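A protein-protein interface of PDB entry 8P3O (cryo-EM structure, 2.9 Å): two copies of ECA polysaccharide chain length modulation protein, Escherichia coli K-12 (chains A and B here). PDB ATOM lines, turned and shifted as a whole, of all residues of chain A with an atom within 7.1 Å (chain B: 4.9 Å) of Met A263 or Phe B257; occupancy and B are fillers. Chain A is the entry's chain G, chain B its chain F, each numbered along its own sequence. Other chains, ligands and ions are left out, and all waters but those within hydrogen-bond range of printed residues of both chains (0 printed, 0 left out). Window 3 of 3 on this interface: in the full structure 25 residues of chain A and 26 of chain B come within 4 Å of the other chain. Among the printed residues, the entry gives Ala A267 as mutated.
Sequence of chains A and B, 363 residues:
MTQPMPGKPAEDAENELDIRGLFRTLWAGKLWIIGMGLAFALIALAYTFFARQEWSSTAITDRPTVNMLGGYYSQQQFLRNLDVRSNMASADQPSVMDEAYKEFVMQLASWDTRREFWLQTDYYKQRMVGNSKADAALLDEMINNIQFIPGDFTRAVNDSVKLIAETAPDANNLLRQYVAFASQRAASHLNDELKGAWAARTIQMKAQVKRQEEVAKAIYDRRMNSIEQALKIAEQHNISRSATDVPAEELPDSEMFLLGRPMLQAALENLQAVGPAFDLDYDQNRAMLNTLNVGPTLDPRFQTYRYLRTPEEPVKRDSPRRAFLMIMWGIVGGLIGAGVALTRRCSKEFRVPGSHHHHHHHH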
ATOM      1  N   LEU A 231      19.350  29.072   0.498  1.00  0.00           N
ATOM      2  CA  LEU A 231      18.482  30.097   1.069  1.00  0.00           C
ATOM      3  C   LEU A 231      19.205  31.433   1.183  1.00  0.00           C
ATOM      4  O   LEU A 231      18.614  32.490   0.931  1.00  0.00           O
ATOM      5  CB  LEU A 231      17.967  29.651   2.435  1.00  0.00           C
ATOM      6  CG  LEU A 231      16.619  28.930   2.454  1.00  0.00           C
ATOM      7  CD1 LEU A 231      16.554  27.948   3.610  1.00  0.00           C
ATOM      8  CD2 LEU A 231      15.480  29.934   2.534  1.00  0.00           C
ATOM      9  N   LEU A 251       4.034  30.863  -8.449  1.00  0.00           N
ATOM     10  CA  LEU A 251       4.633  29.820  -7.623  1.00  0.00           C
ATOM     11  C   LEU A 251       4.302  28.407  -8.105  1.00  0.00           C
ATOM     12  O   LEU A 251       5.203  27.561  -8.141  1.00  0.00           O
ATOM     13  CB  LEU A 251       4.213  29.994  -6.161  1.00  0.00           C
ATOM     14  CG  LEU A 251       4.811  31.200  -5.435  1.00  0.00           C
ATOM     15  CD1 LEU A 251       4.205  31.350  -4.048  1.00  0.00           C
ATOM     16  CD2 LEU A 251       6.326  31.078  -5.352  1.00  0.00           C
ATOM     17  N   MET A 256      11.971  27.296 -11.951  1.00  0.00           N
ATOM     18  CA  MET A 256      12.931  27.785 -10.965  1.00  0.00           C
ATOM     19  C   MET A 256      12.242  28.610  -9.885  1.00  0.00           C
ATOM     20  O   MET A 256      12.611  28.542  -8.708  1.00  0.00           O
ATOM     21  CB  MET A 256      14.056  28.558 -11.677  1.00  0.00           C
ATOM     22  CG  MET A 256      13.856  30.046 -12.052  1.00  0.00           C
ATOM     23  SD  MET A 256      13.468  31.287 -10.794  1.00  0.00           S
ATOM     24  CE  MET A 256      14.801  31.019  -9.627  1.00  0.00           C
ATOM     25  N   PHE A 257      11.232  29.397 -10.266  1.00  0.00           N
ATOM     26  CA  PHE A 257      10.487  30.160  -9.271  1.00  0.00           C
ATOM     27  C   PHE A 257       9.583  29.272  -8.428  1.00  0.00           C
ATOM     28  O   PHE A 257       9.237  29.652  -7.304  1.00  0.00           O
ATOM     29  CB  PHE A 257       9.668  31.258  -9.945  1.00  0.00           C
ATOM     30  CG  PHE A 257       9.448  32.465  -9.078  1.00  0.00           C
ATOM     31  CD1 PHE A 257      10.431  33.433  -8.961  1.00  0.00           C
ATOM     32  CD2 PHE A 257       8.265  32.625  -8.376  1.00  0.00           C
ATOM     33  CE1 PHE A 257      10.237  34.544  -8.165  1.00  0.00           C
ATOM     34  CE2 PHE A 257       8.067  33.735  -7.576  1.00  0.00           C
ATOM     35  CZ  PHE A 257       9.053  34.695  -7.471  1.00  0.00           C
ATOM     36  N   LEU A 258       9.185  28.107  -8.946  1.00  0.00           N
ATOM     37  CA  LEU A 258       8.497  27.130  -8.110  1.00  0.00           C
ATOM     38  C   LEU A 258       9.402  26.668  -6.976  1.00  0.00           C
ATOM     39  O   LEU A 258       8.936  26.414  -5.861  1.00  0.00           O
ATOM     40  CB  LEU A 258       8.030  25.945  -8.957  1.00  0.00           C
ATOM     41  CG  LEU A 258       7.770  24.606  -8.260  1.00  0.00           C
ATOM     42  CD1 LEU A 258       6.584  24.705  -7.308  1.00  0.00           C
ATOM     43  CD2 LEU A 258       7.546  23.503  -9.282  1.00  0.00           C
ATOM     44  N   LEU A 259      10.703  26.557  -7.245  1.00  0.00           N
ATOM     45  CA  LEU A 259      11.691  26.306  -6.196  1.00  0.00           C
ATOM     46  C   LEU A 259      12.303  27.638  -5.757  1.00  0.00           C
ATOM     47  O   LEU A 259      13.482  27.933  -5.965  1.00  0.00           O
ATOM     48  CB  LEU A 259      12.746  25.318  -6.676  1.00  0.00           C
ATOM     49  CG  LEU A 259      12.464  23.853  -6.324  1.00  0.00           C
ATOM     50  CD1 LEU A 259      11.265  23.318  -7.096  1.00  0.00           C
ATOM     51  CD2 LEU A 259      13.694  22.988  -6.563  1.00  0.00           C
ATOM     52  N   GLY A 260      11.454  28.453  -5.134  1.00  0.00           N
ATOM     53  CA  GLY A 260      11.830  29.774  -4.668  1.00  0.00           C
ATOM     54  C   GLY A 260      12.071  29.850  -3.173  1.00  0.00           C
ATOM     55  O   GLY A 260      12.677  28.948  -2.590  1.00  0.00           O
ATOM     56  N   ARG A 261      11.613  30.933  -2.544  1.00  0.00           N
ATOM     57  CA  ARG A 261      11.897  31.140  -1.124  1.00  0.00           C
ATOM     58  C   ARG A 261      11.064  30.253  -0.201  1.00  0.00           C
ATOM     59  O   ARG A 261      11.661  29.521   0.607  1.00  0.00           O
ATOM     60  CB  ARG A 261      11.738  32.629  -0.785  1.00  0.00           C
ATOM     61  CG  ARG A 261      11.311  32.923   0.649  1.00  0.00           C
ATOM     62  CD  ARG A 261      12.443  32.669   1.639  1.00  0.00           C
ATOM     63  NE  ARG A 261      12.072  33.023   3.005  1.00  0.00           N
ATOM     64  CZ  ARG A 261      11.229  32.331   3.760  1.00  0.00           C
ATOM     65  NH1 ARG A 261      10.649  31.227   3.319  1.00  0.00           N
ATOM     66  NH2 ARG A 261      10.967  32.754   4.994  1.00  0.00           N
ATOM     67  N   PRO A 262       9.707  30.257  -0.248  1.00  0.00           N
ATOM     68  CA  PRO A 262       8.946  29.578   0.816  1.00  0.00           C
ATOM     69  C   PRO A 262       9.130  28.067   0.895  1.00  0.00           C
ATOM     70  O   PRO A 262       9.405  27.549   1.981  1.00  0.00           O
ATOM     71  CB  PRO A 262       7.489  29.942   0.495  1.00  0.00           C
ATOM     72  CG  PRO A 262       7.480  30.317  -0.928  1.00  0.00           C
ATOM     73  CD  PRO A 262       8.814  30.934  -1.205  1.00  0.00           C
ATOM     74  N   MET A 263       8.975  27.340  -0.217  1.00  0.00           N
ATOM     75  CA  MET A 263       9.135  25.890  -0.151  1.00  0.00           C
ATOM     76  C   MET A 263      10.573  25.497   0.172  1.00  0.00           C
ATOM     77  O   MET A 263      10.808  24.402   0.693  1.00  0.00           O
ATOM     78  CB  MET A 263       8.682  25.195  -1.444  1.00  0.00           C
ATOM     79  CG  MET A 263       9.596  25.309  -2.668  1.00  0.00           C
ATOM     80  SD  MET A 263      10.427  26.863  -3.034  1.00  0.00           S
ATOM     81  CE  MET A 263       9.045  28.003  -3.109  1.00  0.00           C
ATOM     82  N   LEU A 264      11.543  26.363  -0.132  1.00  0.00           N
ATOM     83  CA  LEU A 264      12.907  26.117   0.323  1.00  0.00           C
ATOM     84  C   LEU A 264      12.972  26.092   1.845  1.00  0.00           C
ATOM     85  O   LEU A 264      13.666  25.253   2.432  1.00  0.00           O
ATOM     86  CB  LEU A 264      13.853  27.181  -0.234  1.00  0.00           C
ATOM     87  CG  LEU A 264      14.773  26.760  -1.382  1.00  0.00           C
ATOM     88  CD1 LEU A 264      15.963  27.701  -1.489  1.00  0.00           C
ATOM     89  CD2 LEU A 264      15.239  25.326  -1.204  1.00  0.00           C
ATOM     90  N   GLN A 265      12.253  27.007   2.497  1.00  0.00           N
ATOM     91  CA  GLN A 265      12.117  26.948   3.949  1.00  0.00           C
ATOM     92  C   GLN A 265      11.409  25.671   4.380  1.00  0.00           C
ATOM     93  O   GLN A 265      11.767  25.067   5.398  1.00  0.00           O
ATOM     94  CB  GLN A 265      11.359  28.178   4.449  1.00  0.00           C
ATOM     95  CG  GLN A 265      11.168  28.232   5.955  1.00  0.00           C
ATOM     96  CD  GLN A 265      12.463  28.037   6.714  1.00  0.00           C
ATOM     97  OE1 GLN A 265      12.606  27.090   7.487  1.00  0.00           O
ATOM     98  NE2 GLN A 265      13.415  28.936   6.498  1.00  0.00           N
ATOM     99  N   ALA A 266      10.399  25.248   3.616  1.00  0.00           N
ATOM    100  CA  ALA A 266       9.682  24.019   3.938  1.00  0.00           C
ATOM    101  C   ALA A 266      10.599  22.804   3.861  1.00  0.00           C
ATOM    102  O   ALA A 266      10.500  21.893   4.692  1.00  0.00           O
ATOM    103  CB  ALA A 266       8.486  23.850   3.003  1.00  0.00           C
ATOM    104  N   ALA A 267      11.488  22.769   2.865  1.00  0.00           N
ATOM    105  CA  ALA A 267      12.407  21.642   2.735  1.00  0.00           C
ATOM    106  C   ALA A 267      13.318  21.526   3.948  1.00  0.00           C
ATOM    107  O   ALA A 267      13.584  20.419   4.432  1.00  0.00           O
ATOM    108  CB  ALA A 267      13.237  21.786   1.460  1.00  0.00           C
ATOM    109  N   LEU A 268      13.810  22.660   4.450  1.00  0.00           N
ATOM    110  CA  LEU A 268      14.678  22.636   5.622  1.00  0.00           C
ATOM    111  C   LEU A 268      13.948  22.091   6.842  1.00  0.00           C
ATOM    112  O   LEU A 268      14.506  21.293   7.604  1.00  0.00           O
ATOM    113  CB  LEU A 268      15.218  24.038   5.900  1.00  0.00           C
ATOM    114  CG  LEU A 268      16.093  24.202   7.143  1.00  0.00           C
ATOM    115  CD1 LEU A 268      17.399  23.444   6.982  1.00  0.00           C
ATOM    116  CD2 LEU A 268      16.353  25.673   7.420  1.00  0.00           C
ATOM    117  N   GLU A 269      12.697  22.512   7.046  1.00  0.00           N
ATOM    118  CA  GLU A 269      11.937  22.054   8.205  1.00  0.00           C
ATOM    119  C   GLU A 269      11.661  20.558   8.138  1.00  0.00           C
ATOM    120  O   GLU A 269      11.781  19.855   9.148  1.00  0.00           O
ATOM    121  CB  GLU A 269      10.627  22.832   8.310  1.00  0.00           C
ATOM    122  CG  GLU A 269      10.584  23.842   9.443  1.00  0.00           C
ATOM    123  CD  GLU A 269       9.695  25.028   9.127  1.00  0.00           C
ATOM    124  OE1 GLU A 269       8.947  24.962   8.128  1.00  0.00           O
ATOM    125  OE2 GLU A 269       9.741  26.026   9.876  1.00  0.00           O
ATOM    126  N   ASN A 270      11.284  20.054   6.961  1.00  0.00           N
ATOM    127  CA  ASN A 270      10.906  18.649   6.842  1.00  0.00           C
ATOM    128  C   ASN A 270      12.100  17.729   7.060  1.00  0.00           C
ATOM    129  O   ASN A 270      12.010  16.756   7.817  1.00  0.00           O
ATOM    130  CB  ASN A 270      10.267  18.395   5.478  1.00  0.00           C
ATOM    131  CG  ASN A 270       9.838  16.954   5.294  1.00  0.00           C
ATOM    132  OD1 ASN A 270       9.558  16.246   6.261  1.00  0.00           O
ATOM    133  ND2 ASN A 270       9.772  16.514   4.044  1.00  0.00           N
ATOM    134  N   LEU A 271      13.224  18.015   6.402  1.00  0.00           N
ATOM    135  CA  LEU A 271      14.412  17.190   6.572  1.00  0.00           C
ATOM    136  C   LEU A 271      14.984  17.297   7.980  1.00  0.00           C
ATOM    137  O   LEU A 271      15.573  16.330   8.473  1.00  0.00           O
ATOM    138  CB  LEU A 271      15.460  17.578   5.525  1.00  0.00           C
ATOM    139  CG  LEU A 271      16.940  17.255   5.733  1.00  0.00           C
ATOM    140  CD1 LEU A 271      17.175  15.753   5.762  1.00  0.00           C
ATOM    141  CD2 LEU A 271      17.765  17.899   4.633  1.00  0.00           C
ATOM    142  N   ALA B 230       5.296  15.193   7.761  1.00  0.00           N
ATOM    143  CA  ALA B 230       5.111  15.936   6.521  1.00  0.00           C
ATOM    144  C   ALA B 230       3.699  16.486   6.377  1.00  0.00           C
ATOM    145  O   ALA B 230       3.503  17.474   5.661  1.00  0.00           O
ATOM    146  CB  ALA B 230       5.447  15.053   5.322  1.00  0.00           C
ATOM    147  N   ILE B 233       3.501  20.008   8.229  1.00  0.00           N
ATOM    148  CA  ILE B 233       4.193  21.076   7.514  1.00  0.00           C
ATOM    149  C   ILE B 233       3.384  21.525   6.303  1.00  0.00           C
ATOM    150  O   ILE B 233       3.289  22.725   6.015  1.00  0.00           O
ATOM    151  CB  ILE B 233       5.607  20.615   7.119  1.00  0.00           C
ATOM    152  CG1 ILE B 233       6.497  20.560   8.360  1.00  0.00           C
ATOM    153  CG2 ILE B 233       6.204  21.538   6.070  1.00  0.00           C
ATOM    154  CD1 ILE B 233       7.897  20.090   8.081  1.00  0.00           C
ATOM    155  N   ILE B 239       0.239  24.198   1.136  1.00  0.00           N
ATOM    156  CA  ILE B 239       0.600  23.660  -0.169  1.00  0.00           C
ATOM    157  C   ILE B 239      -0.362  22.518  -0.473  1.00  0.00           C
ATOM    158  O   ILE B 239      -0.490  21.571   0.311  1.00  0.00           O
ATOM    159  CB  ILE B 239       2.063  23.196  -0.215  1.00  0.00           C
ATOM    160  CG1 ILE B 239       2.334  22.409  -1.500  1.00  0.00           C
ATOM    161  CG2 ILE B 239       2.422  22.387   1.025  1.00  0.00           C
ATOM    162  CD1 ILE B 239       3.800  22.126  -1.744  1.00  0.00           C
ATOM    163  N   SER B 254      13.062  12.018   3.161  1.00  0.00           N
ATOM    164  CA  SER B 254      13.120  13.459   3.380  1.00  0.00           C
ATOM    165  C   SER B 254      11.915  14.163   2.768  1.00  0.00           C
ATOM    166  O   SER B 254      11.155  14.845   3.464  1.00  0.00           O
ATOM    167  CB  SER B 254      14.416  14.018   2.794  1.00  0.00           C
ATOM    168  OG  SER B 254      14.772  15.238   3.411  1.00  0.00           O
ATOM    169  N   GLU B 255      11.725  14.006   1.462  1.00  0.00           N
ATOM    170  CA  GLU B 255      10.873  14.897   0.671  1.00  0.00           C
ATOM    171  C   GLU B 255       9.452  14.379   0.445  1.00  0.00           C
ATOM    172  O   GLU B 255       9.059  14.139  -0.696  1.00  0.00           O
ATOM    173  CB  GLU B 255      11.558  15.184  -0.660  1.00  0.00           C
ATOM    174  CG  GLU B 255      12.357  14.011  -1.206  1.00  0.00           C
ATOM    175  CD  GLU B 255      13.394  14.436  -2.230  1.00  0.00           C
ATOM    176  OE1 GLU B 255      14.168  15.369  -1.934  1.00  0.00           O
ATOM    177  OE2 GLU B 255      13.436  13.840  -3.326  1.00  0.00           O
ATOM    178  N   MET B 256       8.655  14.189   1.500  1.00  0.00           N
ATOM    179  CA  MET B 256       7.215  14.083   1.275  1.00  0.00           C
ATOM    180  C   MET B 256       6.529  15.436   1.171  1.00  0.00           C
ATOM    181  O   MET B 256       5.379  15.488   0.722  1.00  0.00           O
ATOM    182  CB  MET B 256       6.487  13.265   2.357  1.00  0.00           C
ATOM    183  CG  MET B 256       6.427  11.732   2.195  1.00  0.00           C
ATOM    184  SD  MET B 256       7.801  10.739   1.609  1.00  0.00           S
ATOM    185  CE  MET B 256       9.115  11.435   2.570  1.00  0.00           C
ATOM    186  N   PHE B 257       7.188  16.525   1.571  1.00  0.00           N
ATOM    187  CA  PHE B 257       6.549  17.831   1.474  1.00  0.00           C
ATOM    188  C   PHE B 257       6.328  18.258   0.031  1.00  0.00           C
ATOM    189  O   PHE B 257       5.562  19.197  -0.211  1.00  0.00           O
ATOM    190  CB  PHE B 257       7.376  18.897   2.194  1.00  0.00           C
ATOM    191  CG  PHE B 257       8.472  19.485   1.355  1.00  0.00           C
ATOM    192  CD1 PHE B 257       9.494  18.692   0.858  1.00  0.00           C
ATOM    193  CD2 PHE B 257       8.469  20.834   1.045  1.00  0.00           C
ATOM    194  CE1 PHE B 257      10.495  19.237   0.079  1.00  0.00           C
ATOM    195  CE2 PHE B 257       9.466  21.384   0.268  1.00  0.00           C
ATOM    196  CZ  PHE B 257      10.479  20.585  -0.217  1.00  0.00           C
ATOM    197  N   LEU B 258       6.982  17.602  -0.926  1.00  0.00           N
ATOM    198  CA  LEU B 258       6.753  17.888  -2.335  1.00  0.00           C
ATOM    199  C   LEU B 258       5.534  17.119  -2.820  1.00  0.00           C
ATOM    200  O   LEU B 258       5.582  16.446  -3.855  1.00  0.00           O
ATOM    201  CB  LEU B 258       7.985  17.522  -3.160  1.00  0.00           C
ATOM    202  CG  LEU B 258       9.092  18.574  -3.221  1.00  0.00           C
ATOM    203  CD1 LEU B 258      10.091  18.206  -4.301  1.00  0.00           C
ATOM    204  CD2 LEU B 258       8.525  19.967  -3.458  1.00  0.00           C
ATOM    205  N   LEU B 259       4.437  17.231  -2.078  1.00  0.00           N
ATOM    206  CA  LEU B 259       3.170  16.609  -2.421  1.00  0.00           C
ATOM    207  C   LEU B 259       2.060  17.443  -1.804  1.00  0.00           C
ATOM    208  O   LEU B 259       2.248  18.095  -0.773  1.00  0.00           O
ATOM    209  CB  LEU B 259       3.088  15.155  -1.934  1.00  0.00           C
ATOM    210  CG  LEU B 259       3.751  14.062  -2.777  1.00  0.00           C
ATOM    211  CD1 LEU B 259       3.408  12.684  -2.237  1.00  0.00           C
ATOM    212  CD2 LEU B 259       3.339  14.178  -4.237  1.00  0.00           C
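The backbone NH of Gly A260 is in hydrogen-bond range of the side-chain sulfur of Met A263 (2.8 Å).
Of chain B, only Phe B257 (3.3 Å) comes within 4 Å of Met A263. Of the printed residues of chain B, Ala A266 touches Phe B257 (3.6 Å). Of the printed residues of chain B, Ala A267 touches Phe B257. Of chain A, only Met A263 (3.3 Å), Ala A266 (3.6 Å), Ala A267 (3.4 Å) and Asn A270 (3.6 Å) come within 4 Å of Phe B257. The nearest residue of chain A that does not touch Phe B257 is Leu A264 (5.4 Å).
Met A263 touches Phe B257. CB of Ala A266 touches CD2 of Phe B257, 3.6 Å away. CB of Ala A267 touches CZ of Phe B257, 3.4 Å away. CD1 of Ile B233 touches C of Glu A269 (3.8 Å). CD1 of Ile B233 touches CA of Asn A270 (3.6 Å). Glu B255 touches Asn A270 (CA to ND2, 3.9 Å). Met B256 touches Asn A270. Asn A270 touches Phe B257 (ND2 to N, 3.6 Å). CB of Leu A271 touches OG of Ser B254, at 3.2 Å.
The side-chain amide nitrogen of Asn A270 sits close to the backbone carbonyl oxygen of Ser B254 (2.2 Å).
Positions printed for both chains: 256, 257, 258 and 259.
Printed residues of chain B that touch a printed residue of chain A: Ile B233, Ser B254, Glu B255, Met B256 and Phe B257. Hydrophobic or aromatic side chains of chain B within 4 Å of the printed part of chain A: Ile B233 and Phe B257. Of the 18 printed residues of chain A, 6 touch a printed residue of chain B. Among the printed residues, 10 pairs touch across the chains. Among the printed residues, no Asp or Glu carboxylate lies within 4 Å of a Lys or Arg side-chain nitrogen of the other chain.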
